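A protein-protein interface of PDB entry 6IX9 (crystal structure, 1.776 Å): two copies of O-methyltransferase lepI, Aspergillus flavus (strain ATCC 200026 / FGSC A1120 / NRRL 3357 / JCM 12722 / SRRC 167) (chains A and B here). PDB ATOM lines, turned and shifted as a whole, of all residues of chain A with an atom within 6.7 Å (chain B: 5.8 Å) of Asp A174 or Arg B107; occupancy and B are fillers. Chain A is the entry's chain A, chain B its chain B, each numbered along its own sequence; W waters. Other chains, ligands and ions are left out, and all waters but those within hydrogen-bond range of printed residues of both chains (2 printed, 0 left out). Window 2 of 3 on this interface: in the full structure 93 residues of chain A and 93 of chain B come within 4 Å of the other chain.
Water W2 lies within hydrogen-bond range of O of Ile A175 (2.7 Å) and NH1 of Arg B112 (2.8 Å).
Water W1 lies within hydrogen-bond range of N of Arg B107 (2.9 Å) and OD2 of Asp A174 (3.4 Å).
The backbone carbonyl oxygen of Tyr A172 sits at hydrogen-bond distance from the backbone NH of Gly B106 (2.9 Å).
The backbone NH of Glu B108 is in hydrogen-bond range of the side-chain carboxylate of Asp A174.
The side-chain carboxylate of Asp A174 sits at hydrogen-bond distance from the backbone NH of Leu B109.
Of the 12 printed residues of chain B, 6 touch a printed residue of chain A.
Hydrophobic or aromatic side chains of chain B that line the printed part of chain A: Leu B109.
Hydrophobic or aromatic side chains of chain A within 4 Å of the printed part of chain B: Leu A167, Tyr A172 and Met A361.
Among the printed residues, 11 pairs touch across the chains.
Among the printed residues, no Asp or Glu carboxylate lies within 4 Å of a Lys or Arg side-chain nitrogen of the other chain.
Of chain B, only Gly B106, Arg B107, Glu B108 and Leu B109 come within 4 Å of Asp A174.
Arg B107 touches one residue of chain A.
Printed residues of chain A within 4 Å of Glu B108: Asp A174 (3.2 Å).
Printed residues of chain B within 4 Å of Tyr A172: Cys B105 (3.8 Å), Gly B106 (2.9 Å) and Leu B109 (3.8 Å).
Asp A177 touches none of the printed residues of chain B.
Among the printed residues, pairs that only touch across the chains: Leu A167 with Leu B109 (3.9 Å), Tyr A172 with Cys B105 (3.8 Å), Tyr A172 with Leu B109 (3.8 Å), Pro A173 with Leu B109 (3.5 Å), Asp A174 with Gly B106 (3.2 Å), Asp A174 with Arg B107 (3.5 Å), Met A361 with Leu B109 (3.7 Å) and Met A361 with Arg B112 (3.2 Å).
The backbone carbonyl oxygen of Leu A167 lies within hydrogen-bond range of the backbone NH of Tyr A172.
NH1 of Arg B107 lies within salt-bridge range of OE1 of Glu B97 (3.7 Å).
N of Cys B105 is in hydrogen-bond range of O of Ala B100 (3.0 Å).
OD2 of Asp B101 lies within salt-bridge range of NH1 of Arg B107, at 2.8 Å.
SG of Cys B105 is in hydrogen-bond range of N of Met B110, at 3.7 Å.
No position is printed for both chains.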
ATOM      1  N   LEU A 167       5.493 -15.514  -6.308  1.00  0.00           N
ATOM      2  CA  LEU A 167       6.324 -14.444  -5.763  1.00  0.00           C
ATOM      3  C   LEU A 167       5.759 -13.926  -4.447  1.00  0.00           C
ATOM      4  O   LEU A 167       6.516 -13.632  -3.512  1.00  0.00           O
ATOM      5  CB  LEU A 167       6.443 -13.297  -6.771  1.00  0.00           C
ATOM      6  CG  LEU A 167       7.196 -13.606  -8.069  1.00  0.00           C
ATOM      7  CD1 LEU A 167       7.084 -12.413  -9.049  1.00  0.00           C
ATOM      8  CD2 LEU A 167       8.653 -13.957  -7.797  1.00  0.00           C
ATOM      9  N   LYS A 171       7.740 -14.065  -0.768  1.00  0.00           N
ATOM     10  CA  LYS A 171       8.234 -12.723  -0.439  1.00  0.00           C
ATOM     11  C   LYS A 171       9.225 -12.206  -1.489  1.00  0.00           C
ATOM     12  O   LYS A 171      10.267 -11.633  -1.166  1.00  0.00           O
ATOM     13  CB  LYS A 171       8.849 -12.697   0.966  1.00  0.00           C
ATOM     14  CG  LYS A 171       8.061 -13.507   1.986  1.00  0.00           C
ATOM     15  CD  LYS A 171       8.856 -13.699   3.291  1.00  0.00           C
ATOM     16  CE  LYS A 171       8.239 -14.750   4.212  1.00  0.00           C
ATOM     17  NZ  LYS A 171       6.917 -14.321   4.755  1.00  0.00           N
ATOM     18  N   TYR A 172       8.890 -12.402  -2.763  1.00  0.00           N
ATOM     19  CA  TYR A 172       9.542 -11.709  -3.877  1.00  0.00           C
ATOM     20  C   TYR A 172      11.046 -11.966  -3.906  1.00  0.00           C
ATOM     21  O   TYR A 172      11.847 -11.022  -3.883  1.00  0.00           O
ATOM     22  CB  TYR A 172       9.202 -10.209  -3.819  1.00  0.00           C
ATOM     23  CG  TYR A 172       7.692 -10.034  -3.935  1.00  0.00           C
ATOM     24  CD1 TYR A 172       7.059 -10.042  -5.178  1.00  0.00           C
ATOM     25  CD2 TYR A 172       6.894  -9.972  -2.793  1.00  0.00           C
ATOM     26  CE1 TYR A 172       5.688  -9.964  -5.282  1.00  0.00           C
ATOM     27  CE2 TYR A 172       5.524  -9.877  -2.881  1.00  0.00           C
ATOM     28  CZ  TYR A 172       4.918  -9.880  -4.119  1.00  0.00           C
ATOM     29  OH  TYR A 172       3.541  -9.791  -4.189  1.00  0.00           O
ATOM     30  N   PRO A 173      11.462 -13.230  -3.979  1.00  0.00           N
ATOM     31  CA  PRO A 173      12.890 -13.534  -4.058  1.00  0.00           C
ATOM     32  C   PRO A 173      13.445 -13.242  -5.438  1.00  0.00           C
ATOM     33  O   PRO A 173      12.729 -13.221  -6.441  1.00  0.00           O
ATOM     34  CB  PRO A 173      12.929 -15.037  -3.792  1.00  0.00           C
ATOM     35  CG  PRO A 173      11.695 -15.503  -4.518  1.00  0.00           C
ATOM     36  CD  PRO A 173      10.650 -14.435  -4.238  1.00  0.00           C
ATOM     37  N   ASP A 174      14.750 -13.031  -5.477  1.00  0.00           N
ATOM     38  CA  ASP A 174      15.461 -13.080  -6.746  1.00  0.00           C
ATOM     39  C   ASP A 174      15.519 -14.533  -7.194  1.00  0.00           C
ATOM     40  O   ASP A 174      16.039 -15.385  -6.472  1.00  0.00           O
ATOM     41  CB  ASP A 174      16.862 -12.489  -6.596  1.00  0.00           C
ATOM     42  CG  ASP A 174      16.844 -10.977  -6.332  1.00  0.00           C
ATOM     43  OD1 ASP A 174      15.812 -10.337  -6.601  1.00  0.00           O
ATOM     44  OD2 ASP A 174      17.860 -10.418  -5.863  1.00  0.00           O
ATOM     45  N   ILE A 175      14.979 -14.823  -8.371  1.00  0.00           N
ATOM     46  CA  ILE A 175      14.938 -16.190  -8.875  1.00  0.00           C
ATOM     47  C   ILE A 175      16.263 -16.487  -9.568  1.00  0.00           C
ATOM     48  O   ILE A 175      16.664 -15.772 -10.494  1.00  0.00           O
ATOM     49  CB  ILE A 175      13.744 -16.386  -9.822  1.00  0.00           C
ATOM     50  CG1 ILE A 175      12.448 -16.190  -9.027  1.00  0.00           C
ATOM     51  CG2 ILE A 175      13.773 -17.763 -10.468  1.00  0.00           C
ATOM     52  CD1 ILE A 175      11.198 -16.388  -9.820  1.00  0.00           C
ATOM     53  N   VAL A 176      16.962 -17.524  -9.099  1.00  0.00           N
ATOM     54  CA  VAL A 176      18.290 -17.854  -9.602  1.00  0.00           C
ATOM     55  C   VAL A 176      18.461 -19.334  -9.900  1.00  0.00           C
ATOM     56  O   VAL A 176      19.542 -19.744 -10.337  1.00  0.00           O
ATOM     57  CB  VAL A 176      19.385 -17.386  -8.622  1.00  0.00           C
ATOM     58  CG1 VAL A 176      19.362 -15.873  -8.483  1.00  0.00           C
ATOM     59  CG2 VAL A 176      19.184 -18.051  -7.263  1.00  0.00           C
ATOM     60  N   ASP A 177      17.433 -20.156  -9.685  1.00  0.00           N
ATOM     61  CA  ASP A 177      17.564 -21.609  -9.683  1.00  0.00           C
ATOM     62  C   ASP A 177      16.460 -22.207 -10.539  1.00  0.00           C
ATOM     63  O   ASP A 177      15.278 -21.923 -10.309  1.00  0.00           O
ATOM     64  CB  ASP A 177      17.482 -22.140  -8.239  1.00  0.00           C
ATOM     65  CG  ASP A 177      17.436 -23.683  -8.148  1.00  0.00           C
ATOM     66  OD1 ASP A 177      17.612 -24.384  -9.169  1.00  0.00           O
ATOM     67  OD2 ASP A 177      17.206 -24.197  -7.018  1.00  0.00           O
ATOM     68  N   ASP A 180      13.594 -23.867  -8.625  1.00  0.00           N
ATOM     69  CA  ASP A 180      12.825 -23.123  -7.642  1.00  0.00           C
ATOM     70  C   ASP A 180      12.310 -21.851  -8.297  1.00  0.00           C
ATOM     71  O   ASP A 180      12.772 -20.750  -8.018  1.00  0.00           O
ATOM     72  CB  ASP A 180      13.655 -22.803  -6.398  1.00  0.00           C
ATOM     73  CG  ASP A 180      12.812 -22.208  -5.270  1.00  0.00           C
ATOM     74  OD1 ASP A 180      11.557 -22.237  -5.364  1.00  0.00           O
ATOM     75  OD2 ASP A 180      13.406 -21.708  -4.287  1.00  0.00           O
ATOM     76  N   MET A 361      12.624 -16.500 -16.900  1.00  0.00           N
ATOM     77  CA  MET A 361      12.804 -16.524 -15.444  1.00  0.00           C
ATOM     78  C   MET A 361      11.760 -17.420 -14.785  1.00  0.00           C
ATOM     79  O   MET A 361      12.083 -18.258 -13.923  1.00  0.00           O
ATOM     80  CB  MET A 361      12.728 -15.100 -14.874  1.00  0.00           C
ATOM     81  CG  MET A 361      12.693 -15.005 -13.348  1.00  0.00           C
ATOM     82  SD  MET A 361      11.636 -13.626 -12.757  1.00  0.00           S
ATOM     83  CE  MET A 361      12.828 -12.282 -12.604  1.00  0.00           C
ATOM     84  N   ALA B  96      15.610   1.527  -9.325  1.00  0.00           N
ATOM     85  CA  ALA B  96      15.074   0.200  -9.042  1.00  0.00           C
ATOM     86  C   ALA B  96      15.416  -0.225  -7.620  1.00  0.00           C
ATOM     87  O   ALA B  96      14.600  -0.858  -6.939  1.00  0.00           O
ATOM     88  CB  ALA B  96      15.594  -0.820 -10.060  1.00  0.00           C
ATOM     89  N   GLU B  97      16.617   0.141  -7.140  1.00  0.00           N
ATOM     90  CA  GLU B  97      16.949  -0.282  -5.787  1.00  0.00           C
ATOM     91  C   GLU B  97      16.093   0.452  -4.750  1.00  0.00           C
ATOM     92  O   GLU B  97      15.596  -0.163  -3.794  1.00  0.00           O
ATOM     93  CB  GLU B  97      18.448  -0.058  -5.541  1.00  0.00           C
ATOM     94  CG  GLU B  97      18.847   1.368  -5.415  1.00  0.00           C
ATOM     95  CD  GLU B  97      19.982   1.576  -4.424  1.00  0.00           C
ATOM     96  OE1 GLU B  97      21.084   0.999  -4.622  1.00  0.00           O
ATOM     97  OE2 GLU B  97      19.763   2.310  -3.434  1.00  0.00           O
ATOM     98  N   ALA B 100      12.698  -1.300  -4.851  1.00  0.00           N
ATOM     99  CA  ALA B 100      12.788  -2.637  -4.278  1.00  0.00           C
ATOM    100  C   ALA B 100      12.792  -2.583  -2.760  1.00  0.00           C
ATOM    101  O   ALA B 100      12.050  -3.321  -2.099  1.00  0.00           O
ATOM    102  CB  ALA B 100      14.050  -3.340  -4.786  1.00  0.00           C
ATOM    103  N   ASP B 101      13.637  -1.711  -2.187  1.00  0.00           N
ATOM    104  CA  ASP B 101      13.694  -1.708  -0.732  1.00  0.00           C
ATOM    105  C   ASP B 101      12.466  -1.044  -0.127  1.00  0.00           C
ATOM    106  O   ASP B 101      11.969  -1.490   0.905  1.00  0.00           O
ATOM    107  CB  ASP B 101      14.975  -1.007  -0.266  1.00  0.00           C
ATOM    108  CG  ASP B 101      16.251  -1.652  -0.839  1.00  0.00           C
ATOM    109  OD1 ASP B 101      16.226  -2.847  -1.242  1.00  0.00           O
ATOM    110  OD2 ASP B 101      17.285  -0.951  -0.903  1.00  0.00           O
ATOM    111  N   CYS B 105      10.753  -6.000  -2.215  1.00  0.00           N
ATOM    112  CA  CYS B 105      10.967  -6.866  -3.361  1.00  0.00           C
ATOM    113  C   CYS B 105      12.461  -7.103  -3.517  1.00  0.00           C
ATOM    114  O   CYS B 105      13.269  -6.216  -3.233  1.00  0.00           O
ATOM    115  CB  CYS B 105      10.382  -6.216  -4.623  1.00  0.00           C
ATOM    116  SG  CYS B 105      10.518  -7.185  -6.126  1.00  0.00           S
ATOM    117  N   GLY B 106      12.833  -8.305  -3.950  1.00  0.00           N
ATOM    118  CA  GLY B 106      14.232  -8.554  -4.244  1.00  0.00           C
ATOM    119  C   GLY B 106      14.721  -7.574  -5.292  1.00  0.00           C
ATOM    120  O   GLY B 106      13.986  -7.207  -6.205  1.00  0.00           O
ATOM    121  N   ARG B 107      15.974  -7.136  -5.147  1.00  0.00           N
ATOM    122  CA  ARG B 107      16.424  -6.017  -5.974  1.00  0.00           C
ATOM    123  C   ARG B 107      16.581  -6.412  -7.433  1.00  0.00           C
ATOM    124  O   ARG B 107      16.231  -5.635  -8.329  1.00  0.00           O
ATOM    125  CB  ARG B 107      17.741  -5.466  -5.445  1.00  0.00           C
ATOM    126  CG  ARG B 107      17.568  -4.633  -4.213  1.00  0.00           C
ATOM    127  CD  ARG B 107      18.867  -4.494  -3.467  1.00  0.00           C
ATOM    128  NE  ARG B 107      18.876  -3.221  -2.759  1.00  0.00           N
ATOM    129  CZ  ARG B 107      19.930  -2.423  -2.666  1.00  0.00           C
ATOM    130  NH1 ARG B 107      19.836  -1.276  -1.997  1.00  0.00           N
ATOM    131  NH2 ARG B 107      21.070  -2.767  -3.245  1.00  0.00           N
ATOM    132  N   GLU B 108      17.045  -7.629  -7.717  1.00  0.00           N
ATOM    133  CA  GLU B 108      17.175  -8.053  -9.106  1.00  0.00           C
ATOM    134  C   GLU B 108      15.813  -8.286  -9.736  1.00  0.00           C
ATOM    135  O   GLU B 108      15.580  -7.914 -10.896  1.00  0.00           O
ATOM    136  CB  GLU B 108      18.026  -9.321  -9.184  1.00  0.00           C
ATOM    137  CG  GLU B 108      18.303  -9.790 -10.593  1.00  0.00           C
ATOM    138  CD  GLU B 108      19.147  -8.805 -11.389  1.00  0.00           C
ATOM    139  OE1 GLU B 108      19.284  -9.007 -12.618  1.00  0.00           O
ATOM    140  OE2 GLU B 108      19.672  -7.832 -10.793  1.00  0.00           O
ATOM    141  N   LEU B 109      14.909  -8.921  -8.990  1.00  0.00           N
ATOM    142  CA  LEU B 109      13.546  -9.102  -9.469  1.00  0.00           C
ATOM    143  C   LEU B 109      12.909  -7.758  -9.779  1.00  0.00           C
ATOM    144  O   LEU B 109      12.322  -7.572 -10.852  1.00  0.00           O
ATOM    145  CB  LEU B 109      12.724  -9.855  -8.416  1.00  0.00           C
ATOM    146  CG  LEU B 109      11.212  -9.979  -8.623  1.00  0.00           C
ATOM    147  CD1 LEU B 109      10.876 -10.770  -9.876  1.00  0.00           C
ATOM    148  CD2 LEU B 109      10.572 -10.628  -7.392  1.00  0.00           C
ATOM    149  N   MET B 110      13.045  -6.789  -8.867  1.00  0.00           N
ATOM    150  CA  MET B 110      12.458  -5.471  -9.095  1.00  0.00           C
ATOM    151  C   MET B 110      13.024  -4.832 -10.353  1.00  0.00           C
ATOM    152  O   MET B 110      12.278  -4.283 -11.176  1.00  0.00           O
ATOM    153  CB  MET B 110      12.690  -4.567  -7.880  1.00  0.00           C
ATOM    154  CG  MET B 110      12.299  -3.106  -8.104  1.00  0.00           C
ATOM    155  SD  MET B 110      10.686  -2.868  -8.922  1.00  0.00           S
ATOM    156  CE  MET B 110       9.622  -3.170  -7.552  1.00  0.00           C
ATOM    157  N   SER B 111      14.338  -4.912 -10.534  1.00  0.00           N
ATOM    158  CA  SER B 111      14.925  -4.313 -11.721  1.00  0.00           C
ATOM    159  C   SER B 111      14.393  -4.965 -12.993  1.00  0.00           C
ATOM    160  O   SER B 111      14.064  -4.264 -13.956  1.00  0.00           O
ATOM    161  CB  SER B 111      16.444  -4.406 -11.665  1.00  0.00           C
ATOM    162  OG  SER B 111      16.969  -3.900 -12.876  1.00  0.00           O
ATOM    163  N   ARG B 112      14.271  -6.299 -13.013  1.00  0.00           N
ATOM    164  CA  ARG B 112      13.763  -6.977 -14.212  1.00  0.00           C
ATOM    165  C   ARG B 112      12.288  -6.672 -14.462  1.00  0.00           C
ATOM    166  O   ARG B 112      11.856  -6.529 -15.619  1.00  0.00           O
ATOM    167  CB  ARG B 112      13.973  -8.483 -14.071  1.00  0.00           C
ATOM    168  CG  ARG B 112      15.469  -8.833 -13.994  1.00  0.00           C
ATOM    169  CD  ARG B 112      15.709 -10.303 -13.645  1.00  0.00           C
ATOM    170  NE  ARG B 112      15.333 -11.193 -14.740  1.00  0.00           N
ATOM    171  CZ  ARG B 112      15.477 -12.517 -14.702  1.00  0.00           C
ATOM    172  NH1 ARG B 112      15.965 -13.116 -13.613  1.00  0.00           N
ATOM    173  NH2 ARG B 112      15.148 -13.252 -15.752  1.00  0.00           N
HETATM  174  O   HOH W   1      17.593  -8.437  -3.141  1.00  0.00           O
HETATM  175  O   HOH W   2      15.846 -15.908 -13.089  1.00  0.00           O
